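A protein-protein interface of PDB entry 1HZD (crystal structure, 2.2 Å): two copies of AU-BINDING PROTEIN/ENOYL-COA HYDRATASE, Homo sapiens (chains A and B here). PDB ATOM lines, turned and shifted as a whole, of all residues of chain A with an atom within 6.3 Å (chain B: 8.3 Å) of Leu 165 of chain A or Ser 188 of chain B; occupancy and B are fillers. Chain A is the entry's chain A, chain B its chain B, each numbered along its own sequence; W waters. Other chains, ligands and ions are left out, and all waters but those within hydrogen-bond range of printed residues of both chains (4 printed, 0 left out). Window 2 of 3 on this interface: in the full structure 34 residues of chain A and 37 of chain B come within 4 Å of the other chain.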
ATOM      1  N   LEU A 157      -4.025   1.615  16.738  1.00  0.00           N
ATOM      2  CA  LEU A 157      -4.301   1.497  15.312  1.00  0.00           C
ATOM      3  C   LEU A 157      -4.941   0.142  15.012  1.00  0.00           C
ATOM      4  O   LEU A 157      -5.998   0.073  14.395  1.00  0.00           O
ATOM      5  CB  LEU A 157      -3.032   1.696  14.474  1.00  0.00           C
ATOM      6  CG  LEU A 157      -3.293   1.860  12.968  1.00  0.00           C
ATOM      7  CD1 LEU A 157      -4.402   2.871  12.742  1.00  0.00           C
ATOM      8  CD2 LEU A 157      -2.016   2.310  12.253  1.00  0.00           C
ATOM      9  N   ILE A 161      -8.747  -0.093  13.333  1.00  0.00           N
ATOM     10  CA  ILE A 161      -9.017  -0.490  11.950  1.00  0.00           C
ATOM     11  C   ILE A 161      -8.759  -1.959  11.634  1.00  0.00           C
ATOM     12  O   ILE A 161      -8.923  -2.395  10.499  1.00  0.00           O
ATOM     13  CB  ILE A 161      -8.199   0.374  10.950  1.00  0.00           C
ATOM     14  CG1 ILE A 161      -6.698   0.096  11.120  1.00  0.00           C
ATOM     15  CG2 ILE A 161      -8.499   1.845  11.183  1.00  0.00           C
ATOM     16  CD1 ILE A 161      -5.828   0.710  10.049  1.00  0.00           C
ATOM     17  N   GLY A 162      -8.368  -2.724  12.639  1.00  0.00           N
ATOM     18  CA  GLY A 162      -8.090  -4.126  12.410  1.00  0.00           C
ATOM     19  C   GLY A 162      -6.598  -4.383  12.338  1.00  0.00           C
ATOM     20  O   GLY A 162      -5.817  -3.514  11.950  1.00  0.00           O
ATOM     21  N   MET A 163      -6.210  -5.596  12.700  1.00  0.00           N
ATOM     22  CA  MET A 163      -4.817  -6.011  12.717  1.00  0.00           C
ATOM     23  C   MET A 163      -4.131  -5.993  11.347  1.00  0.00           C
ATOM     24  O   MET A 163      -3.049  -5.429  11.189  1.00  0.00           O
ATOM     25  CB  MET A 163      -4.729  -7.415  13.326  1.00  0.00           C
ATOM     26  CG  MET A 163      -3.333  -7.844  13.684  1.00  0.00           C
ATOM     27  SD  MET A 163      -3.307  -9.450  14.496  1.00  0.00           S
ATOM     28  CE  MET A 163      -2.996  -8.963  16.147  1.00  0.00           C
ATOM     29  N   SER A 164      -4.757  -6.607  10.353  1.00  0.00           N
ATOM     30  CA  SER A 164      -4.156  -6.658   9.034  1.00  0.00           C
ATOM     31  C   SER A 164      -3.829  -5.281   8.434  1.00  0.00           C
ATOM     32  O   SER A 164      -2.719  -5.059   7.953  1.00  0.00           O
ATOM     33  CB  SER A 164      -5.050  -7.437   8.071  1.00  0.00           C
ATOM     34  OG  SER A 164      -4.347  -7.669   6.869  1.00  0.00           O
ATOM     35  N   LEU A 165      -4.788  -4.363   8.473  1.00  0.00           N
ATOM     36  CA  LEU A 165      -4.583  -3.031   7.924  1.00  0.00           C
ATOM     37  C   LEU A 165      -3.662  -2.166   8.786  1.00  0.00           C
ATOM     38  O   LEU A 165      -2.952  -1.307   8.264  1.00  0.00           O
ATOM     39  CB  LEU A 165      -5.929  -2.330   7.718  1.00  0.00           C
ATOM     40  CG  LEU A 165      -6.858  -3.006   6.697  1.00  0.00           C
ATOM     41  CD1 LEU A 165      -8.262  -2.404   6.804  1.00  0.00           C
ATOM     42  CD2 LEU A 165      -6.289  -2.846   5.277  1.00  0.00           C
ATOM     43  N   ALA A 166      -3.667  -2.377  10.098  1.00  0.00           N
ATOM     44  CA  ALA A 166      -2.790  -1.587  10.951  1.00  0.00           C
ATOM     45  C   ALA A 166      -1.348  -2.031  10.694  1.00  0.00           C
ATOM     46  O   ALA A 166      -0.421  -1.223  10.718  1.00  0.00           O
ATOM     47  CB  ALA A 166      -3.155  -1.771  12.422  1.00  0.00           C
ATOM     48  N   LYS A 167      -1.167  -3.322  10.442  1.00  0.00           N
ATOM     49  CA  LYS A 167       0.156  -3.863  10.164  1.00  0.00           C
ATOM     50  C   LYS A 167       0.682  -3.327   8.832  1.00  0.00           C
ATOM     51  O   LYS A 167       1.812  -2.826   8.758  1.00  0.00           O
ATOM     52  CB  LYS A 167       0.110  -5.393  10.106  1.00  0.00           C
ATOM     53  CG  LYS A 167       0.031  -6.082  11.469  1.00  0.00           C
ATOM     54  CD  LYS A 167      -0.012  -7.587  11.280  1.00  0.00           C
ATOM     55  CE  LYS A 167      -0.143  -8.337  12.606  1.00  0.00           C
ATOM     56  NZ  LYS A 167      -0.376  -9.793  12.361  1.00  0.00           N
ATOM     57  N   GLU A 168      -0.135  -3.428   7.785  1.00  0.00           N
ATOM     58  CA  GLU A 168       0.289  -2.959   6.475  1.00  0.00           C
ATOM     59  C   GLU A 168       0.702  -1.490   6.523  1.00  0.00           C
ATOM     60  O   GLU A 168       1.722  -1.115   5.955  1.00  0.00           O
ATOM     61  CB  GLU A 168      -0.819  -3.157   5.430  1.00  0.00           C
ATOM     62  CG  GLU A 168      -0.357  -2.847   4.005  1.00  0.00           C
ATOM     63  CD  GLU A 168      -1.400  -3.171   2.940  1.00  0.00           C
ATOM     64  OE1 GLU A 168      -2.055  -4.224   3.035  1.00  0.00           O
ATOM     65  OE2 GLU A 168      -1.551  -2.374   1.990  1.00  0.00           O
ATOM     66  N   LEU A 169      -0.079  -0.665   7.214  1.00  0.00           N
ATOM     67  CA  LEU A 169       0.231   0.759   7.310  1.00  0.00           C
ATOM     68  C   LEU A 169       1.550   0.976   8.051  1.00  0.00           C
ATOM     69  O   LEU A 169       2.407   1.732   7.601  1.00  0.00           O
ATOM     70  CB  LEU A 169      -0.903   1.526   8.020  1.00  0.00           C
ATOM     71  CG  LEU A 169      -2.249   1.615   7.287  1.00  0.00           C
ATOM     72  CD1 LEU A 169      -3.246   2.448   8.106  1.00  0.00           C
ATOM     73  CD2 LEU A 169      -2.042   2.251   5.914  1.00  0.00           C
ATOM     74  N   ILE A 170       1.720   0.303   9.182  1.00  0.00           N
ATOM     75  CA  ILE A 170       2.947   0.458   9.953  1.00  0.00           C
ATOM     76  C   ILE A 170       4.164  -0.127   9.226  1.00  0.00           C
ATOM     77  O   ILE A 170       5.250   0.458   9.266  1.00  0.00           O
ATOM     78  CB  ILE A 170       2.772  -0.160  11.365  1.00  0.00           C
ATOM     79  CG1 ILE A 170       1.809   0.724  12.175  1.00  0.00           C
ATOM     80  CG2 ILE A 170       4.109  -0.268  12.085  1.00  0.00           C
ATOM     81  CD1 ILE A 170       1.546   0.242  13.599  1.00  0.00           C
ATOM     82  N   VAL A 184     -10.786   3.095   5.431  1.00  0.00           N
ATOM     83  CA  VAL A 184     -10.300   2.039   6.327  1.00  0.00           C
ATOM     84  C   VAL A 184     -10.901   2.154   7.724  1.00  0.00           C
ATOM     85  O   VAL A 184     -10.647   1.314   8.589  1.00  0.00           O
ATOM     86  CB  VAL A 184      -8.757   2.035   6.447  1.00  0.00           C
ATOM     87  CG1 VAL A 184      -8.136   1.818   5.083  1.00  0.00           C
ATOM     88  CG2 VAL A 184      -8.266   3.331   7.066  1.00  0.00           C
ATOM     89  N   ILE B 109       2.853 -12.386   3.749  1.00  0.00           N
ATOM     90  CA  ILE B 109       1.776 -12.134   2.812  1.00  0.00           C
ATOM     91  C   ILE B 109       1.332 -13.397   2.097  1.00  0.00           C
ATOM     92  O   ILE B 109       2.149 -14.109   1.490  1.00  0.00           O
ATOM     93  CB  ILE B 109       2.190 -11.097   1.735  1.00  0.00           C
ATOM     94  CG1 ILE B 109       2.662  -9.799   2.401  1.00  0.00           C
ATOM     95  CG2 ILE B 109       1.002 -10.804   0.821  1.00  0.00           C
ATOM     96  CD1 ILE B 109       3.184  -8.752   1.421  1.00  0.00           C
ATOM     97  N   ALA B 110       0.035 -13.676   2.184  1.00  0.00           N
ATOM     98  CA  ALA B 110      -0.543 -14.835   1.519  1.00  0.00           C
ATOM     99  C   ALA B 110      -1.034 -14.380   0.151  1.00  0.00           C
ATOM    100  O   ALA B 110      -1.790 -13.410   0.037  1.00  0.00           O
ATOM    101  CB  ALA B 110      -1.711 -15.391   2.329  1.00  0.00           C
ATOM    102  N   ASP B 128       0.155 -12.026   7.915  1.00  0.00           N
ATOM    103  CA  ASP B 128      -0.229 -10.683   8.330  1.00  0.00           C
ATOM    104  C   ASP B 128      -1.178 -10.021   7.346  1.00  0.00           C
ATOM    105  O   ASP B 128      -2.080  -9.281   7.756  1.00  0.00           O
ATOM    106  CB  ASP B 128       0.996  -9.782   8.482  1.00  0.00           C
ATOM    107  CG  ASP B 128       1.995 -10.323   9.469  1.00  0.00           C
ATOM    108  OD1 ASP B 128       1.581 -10.677  10.587  1.00  0.00           O
ATOM    109  OD2 ASP B 128       3.191 -10.384   9.132  1.00  0.00           O
ATOM    110  N   ILE B 129      -0.981 -10.297   6.055  1.00  0.00           N
ATOM    111  CA  ILE B 129      -1.782  -9.681   5.004  1.00  0.00           C
ATOM    112  C   ILE B 129      -2.167 -10.689   3.931  1.00  0.00           C
ATOM    113  O   ILE B 129      -1.371 -11.551   3.555  1.00  0.00           O
ATOM    114  CB  ILE B 129      -0.995  -8.538   4.333  1.00  0.00           C
ATOM    115  CG1 ILE B 129      -0.542  -7.531   5.386  1.00  0.00           C
ATOM    116  CG2 ILE B 129      -1.838  -7.862   3.271  1.00  0.00           C
ATOM    117  CD1 ILE B 129       0.521  -6.542   4.864  1.00  0.00           C
ATOM    118  N   ARG B 130      -3.389 -10.572   3.441  1.00  0.00           N
ATOM    119  CA  ARG B 130      -3.898 -11.466   2.409  1.00  0.00           C
ATOM    120  C   ARG B 130      -4.238 -10.733   1.107  1.00  0.00           C
ATOM    121  O   ARG B 130      -4.898  -9.696   1.113  1.00  0.00           O
ATOM    122  CB  ARG B 130      -5.151 -12.192   2.912  1.00  0.00           C
ATOM    123  CG  ARG B 130      -4.878 -13.321   3.915  1.00  0.00           C
ATOM    124  CD  ARG B 130      -6.120 -13.630   4.722  1.00  0.00           C
ATOM    125  NE  ARG B 130      -6.436 -12.495   5.584  1.00  0.00           N
ATOM    126  CZ  ARG B 130      -5.677 -12.110   6.611  1.00  0.00           C
ATOM    127  NH1 ARG B 130      -4.567 -12.780   6.908  1.00  0.00           N
ATOM    128  NH2 ARG B 130      -6.003 -11.037   7.316  1.00  0.00           N
ATOM    129  N   VAL B 131      -3.770 -11.286  -0.006  1.00  0.00           N
ATOM    130  CA  VAL B 131      -4.039 -10.734  -1.324  1.00  0.00           C
ATOM    131  C   VAL B 131      -4.592 -11.890  -2.143  1.00  0.00           C
ATOM    132  O   VAL B 131      -4.037 -12.992  -2.123  1.00  0.00           O
ATOM    133  CB  VAL B 131      -2.745 -10.170  -1.985  1.00  0.00           C
ATOM    134  CG1 VAL B 131      -1.610 -11.133  -1.812  1.00  0.00           C
ATOM    135  CG2 VAL B 131      -2.972  -9.937  -3.469  1.00  0.00           C
ATOM    136  N   ALA B 132      -5.695 -11.664  -2.847  1.00  0.00           N
ATOM    137  CA  ALA B 132      -6.273 -12.732  -3.654  1.00  0.00           C
ATOM    138  C   ALA B 132      -6.799 -12.265  -5.005  1.00  0.00           C
ATOM    139  O   ALA B 132      -7.109 -11.086  -5.199  1.00  0.00           O
ATOM    140  CB  ALA B 132      -7.406 -13.418  -2.879  1.00  0.00           C
ATOM    141  N   ALA B 160     -10.398 -11.454  12.292  1.00  0.00           N
ATOM    142  CA  ALA B 160     -10.148 -10.752  11.036  1.00  0.00           C
ATOM    143  C   ALA B 160     -11.353 -10.042  10.414  1.00  0.00           C
ATOM    144  O   ALA B 160     -11.196  -8.964   9.856  1.00  0.00           O
ATOM    145  CB  ALA B 160      -9.536 -11.712  10.016  1.00  0.00           C
ATOM    146  N   GLY B 178     -12.917 -14.038  -4.645  1.00  0.00           N
ATOM    147  CA  GLY B 178     -12.073 -12.913  -4.271  1.00  0.00           C
ATOM    148  C   GLY B 178     -12.802 -11.608  -4.016  1.00  0.00           C
ATOM    149  O   GLY B 178     -12.480 -10.896  -3.060  1.00  0.00           O
ATOM    150  N   ALA B 181     -14.571 -11.776  -0.683  1.00  0.00           N
ATOM    151  CA  ALA B 181     -13.601 -11.763   0.409  1.00  0.00           C
ATOM    152  C   ALA B 181     -13.158 -10.338   0.722  1.00  0.00           C
ATOM    153  O   ALA B 181     -13.030  -9.952   1.889  1.00  0.00           O
ATOM    154  CB  ALA B 181     -12.395 -12.616   0.048  1.00  0.00           C
ATOM    155  N   LYS B 182     -12.926  -9.557  -0.326  1.00  0.00           N
ATOM    156  CA  LYS B 182     -12.508  -8.174  -0.161  1.00  0.00           C
ATOM    157  C   LYS B 182     -13.635  -7.388   0.495  1.00  0.00           C
ATOM    158  O   LYS B 182     -13.391  -6.534   1.339  1.00  0.00           O
ATOM    159  CB  LYS B 182     -12.170  -7.555  -1.522  1.00  0.00           C
ATOM    160  CG  LYS B 182     -11.749  -6.089  -1.464  1.00  0.00           C
ATOM    161  CD  LYS B 182     -10.493  -5.922  -0.627  1.00  0.00           C
ATOM    162  CE  LYS B 182      -9.846  -4.562  -0.826  1.00  0.00           C
ATOM    163  NZ  LYS B 182     -10.724  -3.456  -0.402  1.00  0.00           N
ATOM    164  N   ALA B 183     -14.870  -7.691   0.111  1.00  0.00           N
ATOM    165  CA  ALA B 183     -16.035  -6.998   0.656  1.00  0.00           C
ATOM    166  C   ALA B 183     -16.264  -7.247   2.150  1.00  0.00           C
ATOM    167  O   ALA B 183     -16.820  -6.389   2.841  1.00  0.00           O
ATOM    168  CB  ALA B 183     -17.289  -7.374  -0.141  1.00  0.00           C
ATOM    169  N   VAL B 184     -15.856  -8.410   2.651  1.00  0.00           N
ATOM    170  CA  VAL B 184     -16.029  -8.700   4.078  1.00  0.00           C
ATOM    171  C   VAL B 184     -14.720  -8.468   4.825  1.00  0.00           C
ATOM    172  O   VAL B 184     -14.614  -8.730   6.027  1.00  0.00           O
ATOM    173  CB  VAL B 184     -16.505 -10.159   4.325  1.00  0.00           C
ATOM    174  CG1 VAL B 184     -17.840 -10.396   3.639  1.00  0.00           C
ATOM    175  CG2 VAL B 184     -15.479 -11.145   3.826  1.00  0.00           C
ATOM    176  N   GLY B 185     -13.717  -7.973   4.105  1.00  0.00           N
ATOM    177  CA  GLY B 185     -12.430  -7.712   4.719  1.00  0.00           C
ATOM    178  C   GLY B 185     -11.577  -8.939   5.015  1.00  0.00           C
ATOM    179  O   GLY B 185     -10.621  -8.858   5.783  1.00  0.00           O
ATOM    180  N   LEU B 186     -11.914 -10.077   4.424  1.00  0.00           N
ATOM    181  CA  LEU B 186     -11.132 -11.287   4.647  1.00  0.00           C
ATOM    182  C   LEU B 186      -9.731 -11.107   4.045  1.00  0.00           C
ATOM    183  O   LEU B 186      -8.751 -11.697   4.519  1.00  0.00           O
ATOM    184  CB  LEU B 186     -11.841 -12.490   4.019  1.00  0.00           C
ATOM    185  CG  LEU B 186     -11.087 -13.825   4.079  1.00  0.00           C
ATOM    186  CD1 LEU B 186     -10.620 -14.106   5.519  1.00  0.00           C
ATOM    187  CD2 LEU B 186     -12.002 -14.934   3.579  1.00  0.00           C
ATOM    188  N   ILE B 187      -9.650 -10.299   2.988  1.00  0.00           N
ATOM    189  CA  ILE B 187      -8.382  -9.984   2.320  1.00  0.00           C
ATOM    190  C   ILE B 187      -8.320  -8.460   2.197  1.00  0.00           C
ATOM    191  O   ILE B 187      -9.361  -7.784   2.224  1.00  0.00           O
ATOM    192  CB  ILE B 187      -8.295 -10.606   0.896  1.00  0.00           C
ATOM    193  CG1 ILE B 187      -9.377 -10.008  -0.005  1.00  0.00           C
ATOM    194  CG2 ILE B 187      -8.443 -12.125   0.974  1.00  0.00           C
ATOM    195  CD1 ILE B 187      -9.442 -10.634  -1.389  1.00  0.00           C
ATOM    196  N   SER B 188      -7.117  -7.907   2.055  1.00  0.00           N
ATOM    197  CA  SER B 188      -7.000  -6.453   1.949  1.00  0.00           C
ATOM    198  C   SER B 188      -6.734  -5.959   0.523  1.00  0.00           C
ATOM    199  O   SER B 188      -6.808  -4.768   0.247  1.00  0.00           O
ATOM    200  CB  SER B 188      -5.918  -5.946   2.905  1.00  0.00           C
ATOM    201  OG  SER B 188      -4.699  -6.614   2.680  1.00  0.00           O
ATOM    202  N   HIS B 189      -6.436  -6.881  -0.381  1.00  0.00           N
ATOM    203  CA  HIS B 189      -6.178  -6.520  -1.766  1.00  0.00           C
ATOM    204  C   HIS B 189      -6.749  -7.582  -2.673  1.00  0.00           C
ATOM    205  O   HIS B 189      -6.515  -8.781  -2.480  1.00  0.00           O
ATOM    206  CB  HIS B 189      -4.679  -6.401  -2.026  1.00  0.00           C
ATOM    207  CG  HIS B 189      -3.999  -5.401  -1.152  1.00  0.00           C
ATOM    208  ND1 HIS B 189      -4.020  -4.049  -1.416  1.00  0.00           N
ATOM    209  CD2 HIS B 189      -3.308  -5.551   0.001  1.00  0.00           C
ATOM    210  CE1 HIS B 189      -3.370  -3.407  -0.461  1.00  0.00           C
ATOM    211  NE2 HIS B 189      -2.929  -4.296   0.411  1.00  0.00           N
ATOM    212  N   VAL B 190      -7.511  -7.133  -3.660  1.00  0.00           N
ATOM    213  CA  VAL B 190      -8.118  -8.034  -4.617  1.00  0.00           C
ATOM    214  C   VAL B 190      -7.808  -7.494  -6.010  1.00  0.00           C
ATOM    215  O   VAL B 190      -7.680  -6.285  -6.198  1.00  0.00           O
ATOM    216  CB  VAL B 190      -9.659  -8.113  -4.417  1.00  0.00           C
ATOM    217  CG1 VAL B 190     -10.327  -6.776  -4.803  1.00  0.00           C
ATOM    218  CG2 VAL B 190     -10.233  -9.244  -5.245  1.00  0.00           C
ATOM    219  N   LEU B 191      -7.658  -8.394  -6.972  1.00  0.00           N
ATOM    220  CA  LEU B 191      -7.413  -7.999  -8.348  1.00  0.00           C
ATOM    221  C   LEU B 191      -7.752  -9.138  -9.287  1.00  0.00           C
ATOM    222  O   LEU B 191      -7.843 -10.307  -8.894  1.00  0.00           O
ATOM    223  CB  LEU B 191      -5.957  -7.580  -8.579  1.00  0.00           C
ATOM    224  CG  LEU B 191      -4.899  -8.672  -8.735  1.00  0.00           C
ATOM    225  CD1 LEU B 191      -3.699  -8.100  -9.464  1.00  0.00           C
ATOM    226  CD2 LEU B 191      -4.501  -9.223  -7.367  1.00  0.00           C
ATOM    227  N   LYS B 203       1.023  -9.083  -7.153  1.00  0.00           N
ATOM    228  CA  LYS B 203       0.620  -7.981  -6.273  1.00  0.00           C
ATOM    229  C   LYS B 203       1.347  -8.113  -4.921  1.00  0.00           C
ATOM    230  O   LYS B 203       1.890  -7.138  -4.395  1.00  0.00           O
ATOM    231  CB  LYS B 203      -0.904  -7.995  -6.076  1.00  0.00           C
ATOM    232  CG  LYS B 203      -1.438  -7.009  -5.040  1.00  0.00           C
ATOM    233  CD  LYS B 203      -1.003  -5.573  -5.303  1.00  0.00           C
ATOM    234  CE  LYS B 203      -1.545  -4.649  -4.214  1.00  0.00           C
ATOM    235  NZ  LYS B 203      -0.900  -3.309  -4.219  1.00  0.00           N
ATOM    236  N   LEU B 207       3.774  -5.389  -2.956  1.00  0.00           N
ATOM    237  CA  LEU B 207       3.522  -4.928  -1.597  1.00  0.00           C
ATOM    238  C   LEU B 207       4.742  -5.222  -0.715  1.00  0.00           C
ATOM    239  O   LEU B 207       5.177  -4.377   0.072  1.00  0.00           O
ATOM    240  CB  LEU B 207       2.276  -5.622  -1.040  1.00  0.00           C
ATOM    241  CG  LEU B 207       1.883  -5.330   0.408  1.00  0.00           C
ATOM    242  CD1 LEU B 207       1.662  -3.824   0.611  1.00  0.00           C
ATOM    243  CD2 LEU B 207       0.618  -6.127   0.741  1.00  0.00           C
ATOM    244  N   ILE B 226       2.199  -5.488  17.987  1.00  0.00           N
ATOM    245  CA  ILE B 226       0.847  -5.588  17.445  1.00  0.00           C
ATOM    246  C   ILE B 226       0.229  -6.955  17.750  1.00  0.00           C
ATOM    247  O   ILE B 226      -0.854  -7.041  18.348  1.00  0.00           O
ATOM    248  CB  ILE B 226       0.858  -5.308  15.922  1.00  0.00           C
ATOM    249  CG1 ILE B 226       1.261  -3.843  15.689  1.00  0.00           C
ATOM    250  CG2 ILE B 226      -0.517  -5.595  15.297  1.00  0.00           C
ATOM    251  CD1 ILE B 226       1.423  -3.455  14.201  1.00  0.00           C
HETATM  252  O   HOH W   1      -3.642  -5.098   5.069  1.00  0.00           O
HETATM  253  O   HOH W   2      -5.358  -8.991   4.615  1.00  0.00           O
HETATM  254  O   HOH W   3      -2.764  -9.966  10.690  1.00  0.00           O
HETATM  255  O   HOH W   4       0.609 -12.800  12.338  1.00  0.00           O
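CE of Met 163 of chain A touches O of Ile 226 of chain B, 3.6 Å away. Ile 129 of chain B touches Ser 164 of chain A. Arg 130 of chain B touches Ser 164 of chain A (NH2 to OG, 3.8 Å). CD2 of Leu 165 of chain A touches CB of Ser 188 of chain B, at 3.9 Å. Ile 226 of chain B touches Lys 167 of chain A (CG2 to CE, 3.9 Å). CG2 of Ile 129 of chain B touches OE1 of Glu 168 of chain A, 3.7 Å away. Ser 188 of chain B touches Glu 168 of chain A. Leu 207 of chain B touches Glu 168 of chain A (CD1 to OE2, 3.8 Å). Ile 170 of chain A touches Ile 226 of chain B (CD1 to CD1, 3.7 Å).
The backbone NH (N) of Ser 188 of chain B sits at hydrogen-bond distance from the backbone carbonyl oxygen (O) of Arg 130 of chain B, 3.0 Å away. N of Ala 110 of chain B is in hydrogen-bond range of O of Ile 129 of chain B, at 2.9 Å. N of Ala 132 of chain B sits at hydrogen-bond distance from O of His 189 of chain B. The guanidinium group (NE) of Arg 130 of chain B sits at hydrogen-bond distance from the backbone carbonyl oxygen (O) of Leu 186 of chain B. The side-chain amino group (NZ) of Lys 167 of chain A lies within hydrogen-bond range of the side-chain sulfur (SD) of Met 163 of chain A, at 3.6 Å.
NZ of Lys 167 of chain A lies within salt-bridge range of OD1 of Asp 128 of chain B (2.8 Å). The side-chain hydroxyl (OG) of Ser 164 of chain A sits at hydrogen-bond distance from the backbone carbonyl oxygen (O) of Asp 128 of chain B, at 2.9 Å. The side-chain carboxylate of Glu 168 of chain A sits at hydrogen-bond distance from a ring nitrogen (NE2) of His 189 of chain B, 2.8 Å away.
Leu 165 of chain A touches just one residue of chain B: Ser 188. Of the printed residues of chain A, Ser 188 of chain B touches Leu 165 (3.9 Å) and Glu 168 (3.6 Å). Of chain B, only Asp 128, Ile 129 and Arg 130 come within 4 Å of Ser 164 of chain A. No residue of chain B comes within 4 Å of Ala 166 of chain A. Printed residues of chain B within 4 Å of Ile 170 of chain A: Ile 226. Printed residues of chain B within 4 Å of Glu 168 of chain A: Ile 129, Ser 188, His 189 and Leu 207. Of the printed residues of chain B, Lys 167 of chain A touches Asp 128 (2.8 Å) and Ile 226 (3.9 Å). The nearest residue of chain B that does not touch Leu 165 of chain A is Asp 128 of chain B (5.7 Å). The nearest printed residue of chain B that does not touch Glu 168 of chain A is Asp 128 of chain B (6.2 Å).
Of the 12 printed residues of chain A, 6 touch a printed residue of chain B. Hydrophobic or aromatic side chains of chain A that line the printed part of chain B: Met 163, Leu 165 and Ile 170. Of the 23 printed residues of chain B, 7 touch a printed residue of chain A. Printed residues of chain B that touch a printed residue of chain A: Asp 128, Ile 129, Arg 130, Ser 188, His 189, Leu 207 and Ile 226. Hydrophobic or aromatic side chains of chain B that line the printed part of chain A: Ile 129, His 189, Leu 207 and Ile 226. Among the printed residues, 12 pairs touch across the chains. Among the printed residues, Asp or Glu carboxylates within 4 Å of a Lys or Arg side-chain nitrogen of the other chain: Lys 167 of chain A with Asp 128 of chain B.
1 position is printed for both chains. Of the 12 pairs that touch across the chains among the printed residues, none has its exchanged pair printed and touching as well.
Water W1 lies within hydrogen-bond range of the side-chain carboxylate (OE1) of Glu 168 of chain A, the side-chain hydroxyl (OG) of Ser 188 of chain B and the backbone carbonyl oxygen (O) of Ser 164 of chain A. Water W2 lies within hydrogen-bond range of the backbone NH of Arg 130 of chain B (2.8 Å), the side-chain hydroxyl of Ser 164 of chain A (2.8 Å) and the side-chain hydroxyl of Ser 188 of chain B (3.1 Å). Water W4 lies within hydrogen-bond range of OD1 of Asp 128 of chain B (2.9 Å) and NZ of Lys 167 of chain A (3.2 Å). Water W3 lies within hydrogen-bond range of NZ of Lys 167 of chain A (2.9 Å) and O of Asp 128 of chain B (3.1 Å).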
